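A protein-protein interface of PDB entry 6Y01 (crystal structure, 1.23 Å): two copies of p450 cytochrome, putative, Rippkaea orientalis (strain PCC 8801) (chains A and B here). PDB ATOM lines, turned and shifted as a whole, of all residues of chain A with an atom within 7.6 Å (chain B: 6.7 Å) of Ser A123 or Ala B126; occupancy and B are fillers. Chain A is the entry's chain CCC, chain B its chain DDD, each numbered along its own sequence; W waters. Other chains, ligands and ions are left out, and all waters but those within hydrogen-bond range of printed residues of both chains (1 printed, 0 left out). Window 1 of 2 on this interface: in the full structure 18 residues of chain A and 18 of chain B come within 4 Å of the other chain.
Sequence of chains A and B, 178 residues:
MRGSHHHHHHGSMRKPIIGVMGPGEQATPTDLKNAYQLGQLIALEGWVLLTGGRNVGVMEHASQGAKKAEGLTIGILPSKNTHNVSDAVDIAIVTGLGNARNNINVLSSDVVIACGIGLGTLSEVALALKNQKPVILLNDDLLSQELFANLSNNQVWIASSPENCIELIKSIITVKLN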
ATOM      1  N   ASN A  99     -26.114  23.720 -27.787  1.00  0.00           N
ATOM      2  CA  ASN A  99     -24.843  24.280 -27.299  1.00  0.00           C
ATOM      3  C   ASN A  99     -25.049  25.553 -26.452  1.00  0.00           C
ATOM      4  O   ASN A  99     -24.119  25.982 -25.773  1.00  0.00           O
ATOM      5  CB  ASN A  99     -23.867  24.519 -28.435  1.00  0.00           C
ATOM      6  CG  ASN A  99     -23.431  23.260 -29.150  1.00  0.00           C
ATOM      7  OD1 ASN A  99     -23.419  23.210 -30.390  1.00  0.00           O
ATOM      8  ND2 ASN A  99     -23.170  22.243 -28.403  1.00  0.00           N
ATOM      9  N   ARG A 101     -26.483  25.542 -23.773  1.00  0.00           N
ATOM     10  CA  ARG A 101     -26.319  25.161 -22.363  1.00  0.00           C
ATOM     11  C   ARG A 101     -24.917  25.463 -21.841  1.00  0.00           C
ATOM     12  O   ARG A 101     -24.727  25.477 -20.640  1.00  0.00           O
ATOM     13  CB  ARG A 101     -26.674  23.703 -22.099  1.00  0.00           C
ATOM     14  CG  ARG A 101     -25.731  22.606 -22.604  1.00  0.00           C
ATOM     15  CD  ARG A 101     -24.437  22.452 -21.826  1.00  0.00           C
ATOM     16  NE  ARG A 101     -23.988  21.071 -21.878  1.00  0.00           N
ATOM     17  CZ  ARG A 101     -23.378  20.471 -22.857  1.00  0.00           C
ATOM     18  NH1 ARG A 101     -22.927  21.109 -23.904  1.00  0.00           N
ATOM     19  NH2 ARG A 101     -23.209  19.136 -22.786  1.00  0.00           N
ATOM     20  N   ASN A 102     -23.961  25.714 -22.710  1.00  0.00           N
ATOM     21  CA  ASN A 102     -22.574  25.957 -22.306  1.00  0.00           C
ATOM     22  C   ASN A 102     -22.550  27.099 -21.286  1.00  0.00           C
ATOM     23  O   ASN A 102     -21.739  27.120 -20.388  1.00  0.00           O
ATOM     24  CB  ASN A 102     -21.711  26.182 -23.544  1.00  0.00           C
ATOM     25  CG  ASN A 102     -21.554  24.905 -24.372  1.00  0.00           C
ATOM     26  OD1 ASN A 102     -22.165  23.829 -24.079  1.00  0.00           O
ATOM     27  ND2 ASN A 102     -20.737  24.989 -25.454  1.00  0.00           N
ATOM     28  N   ASN A 103     -23.410  28.141 -21.494  1.00  0.00           N
ATOM     29  CA  ASN A 103     -23.402  29.261 -20.554  1.00  0.00           C
ATOM     30  C   ASN A 103     -23.883  28.840 -19.168  1.00  0.00           C
ATOM     31  O   ASN A 103     -23.426  29.394 -18.202  1.00  0.00           O
ATOM     32  CB  ASN A 103     -24.256  30.436 -21.135  1.00  0.00           C
ATOM     33  CG  ASN A 103     -23.765  31.783 -20.615  1.00  0.00           C
ATOM     34  OD1 ASN A 103     -22.541  32.092 -20.528  1.00  0.00           O
ATOM     35  ND2 ASN A 103     -24.726  32.595 -20.195  1.00  0.00           N
ATOM     36  N   VAL A 106     -21.030  27.348 -17.217  1.00  0.00           N
ATOM     37  CA  VAL A 106     -20.070  28.335 -16.721  1.00  0.00           C
ATOM     38  C   VAL A 106     -20.657  29.098 -15.557  1.00  0.00           C
ATOM     39  O   VAL A 106     -19.975  29.347 -14.563  1.00  0.00           O
ATOM     40  CB  VAL A 106     -19.662  29.238 -17.907  1.00  0.00           C
ATOM     41  CG1 VAL A 106     -19.178  30.586 -17.457  1.00  0.00           C
ATOM     42  CG2 VAL A 106     -18.689  28.445 -18.768  1.00  0.00           C
ATOM     43  N   GLY A 118     -11.193  21.400 -27.462  1.00  0.00           N
ATOM     44  CA  GLY A 118     -12.064  21.149 -28.602  1.00  0.00           C
ATOM     45  C   GLY A 118     -12.901  22.408 -28.774  1.00  0.00           C
ATOM     46  O   GLY A 118     -12.794  23.304 -27.923  1.00  0.00           O
ATOM     47  N   LEU A 119     -13.755  22.420 -29.781  1.00  0.00           N
ATOM     48  CA  LEU A 119     -14.523  23.657 -30.080  1.00  0.00           C
ATOM     49  C   LEU A 119     -15.463  24.002 -28.936  1.00  0.00           C
ATOM     50  O   LEU A 119     -15.538  25.176 -28.536  1.00  0.00           O
ATOM     51  CB  LEU A 119     -15.211  23.460 -31.424  1.00  0.00           C
ATOM     52  CG  LEU A 119     -14.257  23.432 -32.611  1.00  0.00           C
ATOM     53  CD1 LEU A 119     -14.977  22.932 -33.866  1.00  0.00           C
ATOM     54  CD2 LEU A 119     -13.656  24.843 -32.862  1.00  0.00           C
ATOM     55  N   GLY A 120     -16.245  23.057 -28.438  1.00  0.00           N
ATOM     56  CA  GLY A 120     -17.169  23.384 -27.352  1.00  0.00           C
ATOM     57  C   GLY A 120     -16.440  23.863 -26.131  1.00  0.00           C
ATOM     58  O   GLY A 120     -16.876  24.797 -25.478  1.00  0.00           O
ATOM     59  N   THR A 121     -15.308  23.232 -25.797  1.00  0.00           N
ATOM     60  CA  THR A 121     -14.538  23.641 -24.631  1.00  0.00           C
ATOM     61  C   THR A 121     -13.988  25.047 -24.830  1.00  0.00           C
ATOM     62  O   THR A 121     -13.987  25.802 -23.854  1.00  0.00           O
ATOM     63  CB  THR A 121     -13.430  22.604 -24.356  1.00  0.00           C
ATOM     64  OG1 THR A 121     -14.023  21.314 -24.197  1.00  0.00           O
ATOM     65  CG2 THR A 121     -12.658  22.934 -23.103  1.00  0.00           C
ATOM     66  N   LEU A 122     -13.525  25.364 -26.037  1.00  0.00           N
ATOM     67  CA  LEU A 122     -13.035  26.746 -26.302  1.00  0.00           C
ATOM     68  C   LEU A 122     -14.149  27.755 -26.015  1.00  0.00           C
ATOM     69  O   LEU A 122     -13.876  28.801 -25.371  1.00  0.00           O
ATOM     70  CB  LEU A 122     -12.638  26.846 -27.757  1.00  0.00           C
ATOM     71  CG  LEU A 122     -11.305  26.297 -28.215  1.00  0.00           C
ATOM     72  CD1 LEU A 122     -11.021  26.898 -29.598  1.00  0.00           C
ATOM     73  CD2 LEU A 122     -10.148  26.670 -27.274  1.00  0.00           C
ATOM     74  N   SER A 123     -15.387  27.432 -26.436  1.00  0.00           N
ATOM     75  CA  SER A 123     -16.536  28.351 -26.215  1.00  0.00           C
ATOM     76  C   SER A 123     -16.746  28.536 -24.709  1.00  0.00           C
ATOM     77  O   SER A 123     -16.990  29.639 -24.249  1.00  0.00           O
ATOM     78  CB  SER A 123     -17.814  27.860 -26.906  1.00  0.00           C
ATOM     79  OG  SER A 123     -18.444  26.735 -26.215  1.00  0.00           O
ATOM     80  N   GLU A 124     -16.678  27.438 -23.937  1.00  0.00           N
ATOM     81  CA  GLU A 124     -16.930  27.506 -22.482  1.00  0.00           C
ATOM     82  C   GLU A 124     -15.832  28.292 -21.767  1.00  0.00           C
ATOM     83  O   GLU A 124     -16.124  29.100 -20.871  1.00  0.00           O
ATOM     84  CB  GLU A 124     -17.049  26.098 -21.872  1.00  0.00           C
ATOM     85  CG  GLU A 124     -18.333  25.434 -22.246  1.00  0.00           C
ATOM     86  CD  GLU A 124     -18.364  23.937 -22.202  1.00  0.00           C
ATOM     87  OE1 GLU A 124     -17.252  23.327 -22.240  1.00  0.00           O
ATOM     88  OE2 GLU A 124     -19.509  23.414 -22.250  1.00  0.00           O
ATOM     89  N   VAL A 125     -14.577  28.061 -22.128  1.00  0.00           N
ATOM     90  CA  VAL A 125     -13.473  28.812 -21.506  1.00  0.00           C
ATOM     91  C   VAL A 125     -13.638  30.292 -21.824  1.00  0.00           C
ATOM     92  O   VAL A 125     -13.492  31.092 -20.919  1.00  0.00           O
ATOM     93  CB  VAL A 125     -12.118  28.289 -21.975  1.00  0.00           C
ATOM     94  CG1 VAL A 125     -10.991  29.217 -21.559  1.00  0.00           C
ATOM     95  CG2 VAL A 125     -11.898  26.860 -21.431  1.00  0.00           C
ATOM     96  N   ALA A 126     -13.940  30.610 -23.074  1.00  0.00           N
ATOM     97  CA  ALA A 126     -14.096  32.028 -23.449  1.00  0.00           C
ATOM     98  C   ALA A 126     -15.211  32.651 -22.621  1.00  0.00           C
ATOM     99  O   ALA A 126     -15.019  33.799 -22.120  1.00  0.00           O
ATOM    100  CB  ALA A 126     -14.309  32.174 -24.934  1.00  0.00           C
ATOM    101  N   LEU A 127     -16.357  31.971 -22.525  1.00  0.00           N
ATOM    102  CA  LEU A 127     -17.490  32.519 -21.739  1.00  0.00           C
ATOM    103  C   LEU A 127     -17.143  32.660 -20.258  1.00  0.00           C
ATOM    104  O   LEU A 127     -17.508  33.613 -19.594  1.00  0.00           O
ATOM    105  CB  LEU A 127     -18.746  31.674 -21.945  1.00  0.00           C
ATOM    106  CG  LEU A 127     -19.357  31.746 -23.351  1.00  0.00           C
ATOM    107  CD1 LEU A 127     -20.441  30.670 -23.534  1.00  0.00           C
ATOM    108  CD2 LEU A 127     -19.879  33.127 -23.619  1.00  0.00           C
ATOM    109  N   ALA A 128     -16.448  31.641 -19.698  1.00  0.00           N
ATOM    110  CA  ALA A 128     -16.078  31.737 -18.304  1.00  0.00           C
ATOM    111  C   ALA A 128     -15.152  32.917 -18.057  1.00  0.00           C
ATOM    112  O   ALA A 128     -15.328  33.631 -17.075  1.00  0.00           O
ATOM    113  CB  ALA A 128     -15.405  30.406 -17.904  1.00  0.00           C
ATOM    114  N   LEU A 129     -14.162  33.099 -18.923  1.00  0.00           N
ATOM    115  CA  LEU A 129     -13.236  34.260 -18.754  1.00  0.00           C
ATOM    116  C   LEU A 129     -13.985  35.592 -18.952  1.00  0.00           C
ATOM    117  O   LEU A 129     -13.700  36.546 -18.208  1.00  0.00           O
ATOM    118  CB  LEU A 129     -12.082  34.097 -19.738  1.00  0.00           C
ATOM    119  CG  LEU A 129     -11.124  32.941 -19.458  1.00  0.00           C
ATOM    120  CD1 LEU A 129     -10.159  32.782 -20.616  1.00  0.00           C
ATOM    121  CD2 LEU A 129     -10.369  33.181 -18.167  1.00  0.00           C
ATOM    122  N   PHE A 148      -5.454  32.188 -24.528  1.00  0.00           N
ATOM    123  CA  PHE A 148      -6.271  32.564 -23.377  1.00  0.00           C
ATOM    124  C   PHE A 148      -5.489  33.396 -22.392  1.00  0.00           C
ATOM    125  O   PHE A 148      -6.108  34.245 -21.752  1.00  0.00           O
ATOM    126  CB  PHE A 148      -6.923  31.352 -22.734  1.00  0.00           C
ATOM    127  CG  PHE A 148      -8.052  30.812 -23.560  1.00  0.00           C
ATOM    128  CD1 PHE A 148      -9.125  31.606 -23.861  1.00  0.00           C
ATOM    129  CD2 PHE A 148      -8.092  29.466 -23.917  1.00  0.00           C
ATOM    130  CE1 PHE A 148     -10.208  31.103 -24.549  1.00  0.00           C
ATOM    131  CE2 PHE A 148      -9.148  28.976 -24.647  1.00  0.00           C
ATOM    132  CZ  PHE A 148     -10.205  29.797 -24.967  1.00  0.00           C
ATOM    133  N   LEU B 119     -12.922  37.681 -26.479  1.00  0.00           N
ATOM    134  CA  LEU B 119     -13.472  36.482 -25.850  1.00  0.00           C
ATOM    135  C   LEU B 119     -14.842  36.119 -26.422  1.00  0.00           C
ATOM    136  O   LEU B 119     -15.117  34.944 -26.714  1.00  0.00           O
ATOM    137  CB  LEU B 119     -13.496  36.702 -24.352  1.00  0.00           C
ATOM    138  CG  LEU B 119     -12.118  36.704 -23.685  1.00  0.00           C
ATOM    139  CD1 LEU B 119     -12.230  37.185 -22.248  1.00  0.00           C
ATOM    140  CD2 LEU B 119     -11.543  35.260 -23.668  1.00  0.00           C
ATOM    141  N   THR B 121     -16.166  36.876 -29.275  1.00  0.00           N
ATOM    142  CA  THR B 121     -15.995  36.481 -30.677  1.00  0.00           C
ATOM    143  C   THR B 121     -15.429  35.068 -30.740  1.00  0.00           C
ATOM    144  O   THR B 121     -15.877  34.282 -31.568  1.00  0.00           O
ATOM    145  CB  THR B 121     -15.124  37.520 -31.399  1.00  0.00           C
ATOM    146  OG1 THR B 121     -15.761  38.826 -31.325  1.00  0.00           O
ATOM    147  CG2 THR B 121     -14.938  37.129 -32.848  1.00  0.00           C
ATOM    148  N   LEU B 122     -14.458  34.777 -29.899  1.00  0.00           N
ATOM    149  CA  LEU B 122     -13.881  33.402 -29.868  1.00  0.00           C
ATOM    150  C   LEU B 122     -14.980  32.385 -29.589  1.00  0.00           C
ATOM    151  O   LEU B 122     -15.027  31.322 -30.267  1.00  0.00           O
ATOM    152  CB  LEU B 122     -12.819  33.318 -28.786  1.00  0.00           C
ATOM    153  CG  LEU B 122     -11.807  32.216 -28.939  1.00  0.00           C
ATOM    154  CD1 LEU B 122     -10.879  32.473 -30.123  1.00  0.00           C
ATOM    155  CD2 LEU B 122     -10.969  32.181 -27.678  1.00  0.00           C
ATOM    156  N   SER B 123     -15.854  32.679 -28.632  1.00  0.00           N
ATOM    157  CA  SER B 123     -16.966  31.748 -28.298  1.00  0.00           C
ATOM    158  C   SER B 123     -17.859  31.547 -29.520  1.00  0.00           C
ATOM    159  O   SER B 123     -18.253  30.421 -29.806  1.00  0.00           O
ATOM    160  CB  SER B 123     -17.759  32.172 -27.080  1.00  0.00           C
ATOM    161  OG  SER B 123     -18.727  33.188 -27.339  1.00  0.00           O
ATOM    162  N   GLU B 124     -18.192  32.639 -30.243  1.00  0.00           N
ATOM    163  CA  GLU B 124     -19.071  32.505 -31.404  1.00  0.00           C
ATOM    164  C   GLU B 124     -18.421  31.739 -32.544  1.00  0.00           C
ATOM    165  O   GLU B 124     -19.095  30.925 -33.174  1.00  0.00           O
ATOM    166  CB  GLU B 124     -19.514  33.897 -31.897  1.00  0.00           C
ATOM    167  CG  GLU B 124     -20.461  34.474 -30.921  1.00  0.00           C
ATOM    168  CD  GLU B 124     -21.300  35.603 -31.314  1.00  0.00           C
ATOM    169  OE1 GLU B 124     -21.680  35.630 -32.565  1.00  0.00           O
ATOM    170  OE2 GLU B 124     -21.717  36.338 -30.403  1.00  0.00           O
ATOM    171  N   VAL B 125     -17.160  32.020 -32.819  1.00  0.00           N
ATOM    172  CA  VAL B 125     -16.453  31.254 -33.875  1.00  0.00           C
ATOM    173  C   VAL B 125     -16.437  29.769 -33.505  1.00  0.00           C
ATOM    174  O   VAL B 125     -16.706  28.963 -34.364  1.00  0.00           O
ATOM    175  CB  VAL B 125     -15.052  31.789 -34.095  1.00  0.00           C
ATOM    176  CG1 VAL B 125     -14.234  30.883 -34.989  1.00  0.00           C
ATOM    177  CG2 VAL B 125     -15.098  33.203 -34.690  1.00  0.00           C
ATOM    178  N   ALA B 126     -16.110  29.471 -32.254  1.00  0.00           N
ATOM    179  CA  ALA B 126     -16.052  28.065 -31.815  1.00  0.00           C
ATOM    180  C   ALA B 126     -17.415  27.401 -32.023  1.00  0.00           C
ATOM    181  O   ALA B 126     -17.478  26.265 -32.548  1.00  0.00           O
ATOM    182  CB  ALA B 126     -15.556  27.986 -30.391  1.00  0.00           C
ATOM    183  N   LEU B 127     -18.489  28.055 -31.579  1.00  0.00           N
ATOM    184  CA  LEU B 127     -19.859  27.508 -31.749  1.00  0.00           C
ATOM    185  C   LEU B 127     -20.216  27.352 -33.229  1.00  0.00           C
ATOM    186  O   LEU B 127     -20.831  26.397 -33.624  1.00  0.00           O
ATOM    187  CB  LEU B 127     -20.888  28.374 -31.017  1.00  0.00           C
ATOM    188  CG  LEU B 127     -20.809  28.352 -29.495  1.00  0.00           C
ATOM    189  CD1 LEU B 127     -21.688  29.458 -28.889  1.00  0.00           C
ATOM    190  CD2 LEU B 127     -21.214  27.011 -28.965  1.00  0.00           C
ATOM    191  N   ALA B 128     -19.875  28.365 -34.047  1.00  0.00           N
ATOM    192  CA  ALA B 128     -20.169  28.248 -35.475  1.00  0.00           C
ATOM    193  C   ALA B 128     -19.457  27.049 -36.084  1.00  0.00           C
ATOM    194  O   ALA B 128     -20.087  26.267 -36.809  1.00  0.00           O
ATOM    195  CB  ALA B 128     -19.758  29.530 -36.185  1.00  0.00           C
ATOM    196  N   LEU B 129     -18.171  26.887 -35.788  1.00  0.00           N
ATOM    197  CA  LEU B 129     -17.424  25.735 -36.357  1.00  0.00           C
ATOM    198  C   LEU B 129     -17.951  24.408 -35.795  1.00  0.00           C
ATOM    199  O   LEU B 129     -18.046  23.474 -36.555  1.00  0.00           O
ATOM    200  CB  LEU B 129     -15.950  25.924 -36.031  1.00  0.00           C
ATOM    201  CG  LEU B 129     -15.265  27.070 -36.773  1.00  0.00           C
ATOM    202  CD1 LEU B 129     -13.881  27.301 -36.229  1.00  0.00           C
ATOM    203  CD2 LEU B 129     -15.215  26.814 -38.257  1.00  0.00           C
ATOM    204  N   LYS B 130     -18.378  24.375 -34.542  1.00  0.00           N
ATOM    205  CA  LYS B 130     -18.940  23.126 -33.958  1.00  0.00           C
ATOM    206  C   LYS B 130     -20.223  22.764 -34.700  1.00  0.00           C
ATOM    207  O   LYS B 130     -20.480  21.586 -34.907  1.00  0.00           O
ATOM    208  CB  LYS B 130     -19.169  23.304 -32.469  1.00  0.00           C
ATOM    209  CG  LYS B 130     -19.682  22.047 -31.767  1.00  0.00           C
ATOM    210  CD  LYS B 130     -19.674  22.195 -30.285  1.00  0.00           C
ATOM    211  CE  LYS B 130     -20.325  20.991 -29.628  1.00  0.00           C
ATOM    212  NZ  LYS B 130     -19.368  19.922 -29.609  1.00  0.00           N
ATOM    213  N   ASN B 131     -21.006  23.770 -35.088  1.00  0.00           N
ATOM    214  CA  ASN B 131     -22.279  23.608 -35.848  1.00  0.00           C
ATOM    215  C   ASN B 131     -22.022  23.447 -37.354  1.00  0.00           C
ATOM    216  O   ASN B 131     -22.989  23.332 -38.088  1.00  0.00           O
ATOM    217  CB  ASN B 131     -23.244  24.739 -35.531  1.00  0.00           C
ATOM    218  CG  ASN B 131     -23.863  24.753 -34.164  1.00  0.00           C
ATOM    219  OD1 ASN B 131     -24.481  23.754 -33.744  1.00  0.00           O
ATOM    220  ND2 ASN B 131     -23.703  25.819 -33.414  1.00  0.00           N
ATOM    221  N   VAL B 135     -17.254  29.831 -41.660  1.00  0.00           N
ATOM    222  CA  VAL B 135     -16.682  30.919 -40.858  1.00  0.00           C
ATOM    223  C   VAL B 135     -15.550  31.555 -41.630  1.00  0.00           C
ATOM    224  O   VAL B 135     -14.674  30.852 -42.116  1.00  0.00           O
ATOM    225  CB  VAL B 135     -16.192  30.461 -39.487  1.00  0.00           C
ATOM    226  CG1 VAL B 135     -15.489  31.598 -38.757  1.00  0.00           C
ATOM    227  CG2 VAL B 135     -17.326  29.902 -38.664  1.00  0.00           C
ATOM    228  N   PHE B 148      -8.056  27.637 -34.804  1.00  0.00           N
ATOM    229  CA  PHE B 148      -9.329  27.284 -35.454  1.00  0.00           C
ATOM    230  C   PHE B 148      -9.105  26.409 -36.695  1.00  0.00           C
ATOM    231  O   PHE B 148      -9.942  25.550 -36.962  1.00  0.00           O
ATOM    232  CB  PHE B 148     -10.131  28.549 -35.759  1.00  0.00           C
ATOM    233  CG  PHE B 148     -10.776  29.116 -34.535  1.00  0.00           C
ATOM    234  CD1 PHE B 148     -11.563  28.322 -33.711  1.00  0.00           C
ATOM    235  CD2 PHE B 148     -10.631  30.449 -34.215  1.00  0.00           C
ATOM    236  CE1 PHE B 148     -12.180  28.832 -32.602  1.00  0.00           C
ATOM    237  CE2 PHE B 148     -11.253  30.979 -33.102  1.00  0.00           C
ATOM    238  CZ  PHE B 148     -12.038  30.168 -32.307  1.00  0.00           C
HETATM  239  O   HOH W   1     -16.708  20.283 -29.441  1.00  0.00           O
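Of the 18 printed residues of chain A, 9 touch a printed residue of chain B.
Among the printed residues, 15 pairs touch across the chains.
Water W1 lies within hydrogen-bond range of the side-chain amino group (NZ) of Lys B130 (2.7 Å) and the backbone NH (N) of Gly A120 (3.0 Å).
Glu A124 touches none of the printed residues of chain B.
Of the printed residues of chain A, Leu B122 touches Phe A148 (3.4 Å).
Of the printed residues of chain A, Ser B123 touches Ser A123 and Leu A127.
Of the printed residues of chain A, Ala B126 touches Leu A119 (3.4 Å) and Ser A123 (3.997 Å).
Printed residues of chain A within 4 Å of Lys B130: Asn A99 (3.3 Å), Leu A119 (3.8 Å) and Gly A120 (3.99 Å).
Of the printed residues of chain A, Phe B148 touches Leu A122.
The nearest printed residue of chain B that does not touch Ser A123 is Leu B122 (5.2 Å).
Among the printed residues, pairs that only touch across the chains: Asn A99 with Lys B130 (3.3 Å), Leu A119 with Ala B126 (3.4 Å), Ala A126 with Leu B119 (3.4 Å), Phe A148 with Leu B122 (3.4 Å), Asn A99 with Asn B131 (3.6 Å), Asn A99 with Leu B127 (3.7 Å), Leu A119 with Lys B130 (3.8 Å), Leu A122 with Phe B148 (3.8 Å), Leu A119 with Leu B129 (3.8 Å), Ser A123 with Ser B123 (3.9 Å), Leu A127 with Ser B123 (3.9 Å), Ser A123 with Leu B127 (3.9 Å), Leu A129 with Leu B119 (3.98 Å), Gly A120 with Lys B130 (3.99 Å) and Ser A123 with Ala B126 (3.997 Å).
Leu A119 touches Ala B126, and with the chains exchanged Ala A126 touches Leu B119.
Leu A119 touches Leu B129, and with the chains exchanged Leu A129 touches Leu B119.
Leu A122 touches Phe B148, and with the chains exchanged Phe A148 touches Leu B122.
Ser A123 touches Leu B127, and with the chains exchanged Leu A127 touches Ser B123.
Positions printed for both chains: 119, 121, 122, 123, 124, 125, 126, 127, 128, 129 and 148.
Of the 15 pairs that touch across the chains among the printed residues, 9 have their exchanged pair printed and touching as well.
The backbone carbonyl oxygen of Gly A120 sits at hydrogen-bond distance from the side-chain hydroxyl of Ser A123, 2.6 Å away.
OG of Ser A123 is in hydrogen-bond range of ND2 of Asn A102 (3.0 Å).
O of Leu B127 lies within hydrogen-bond range of ND2 of Asn B131, at 2.9 Å.
O of Asn A99 sits close to OD1 of Asn A102 (3.4 Å).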
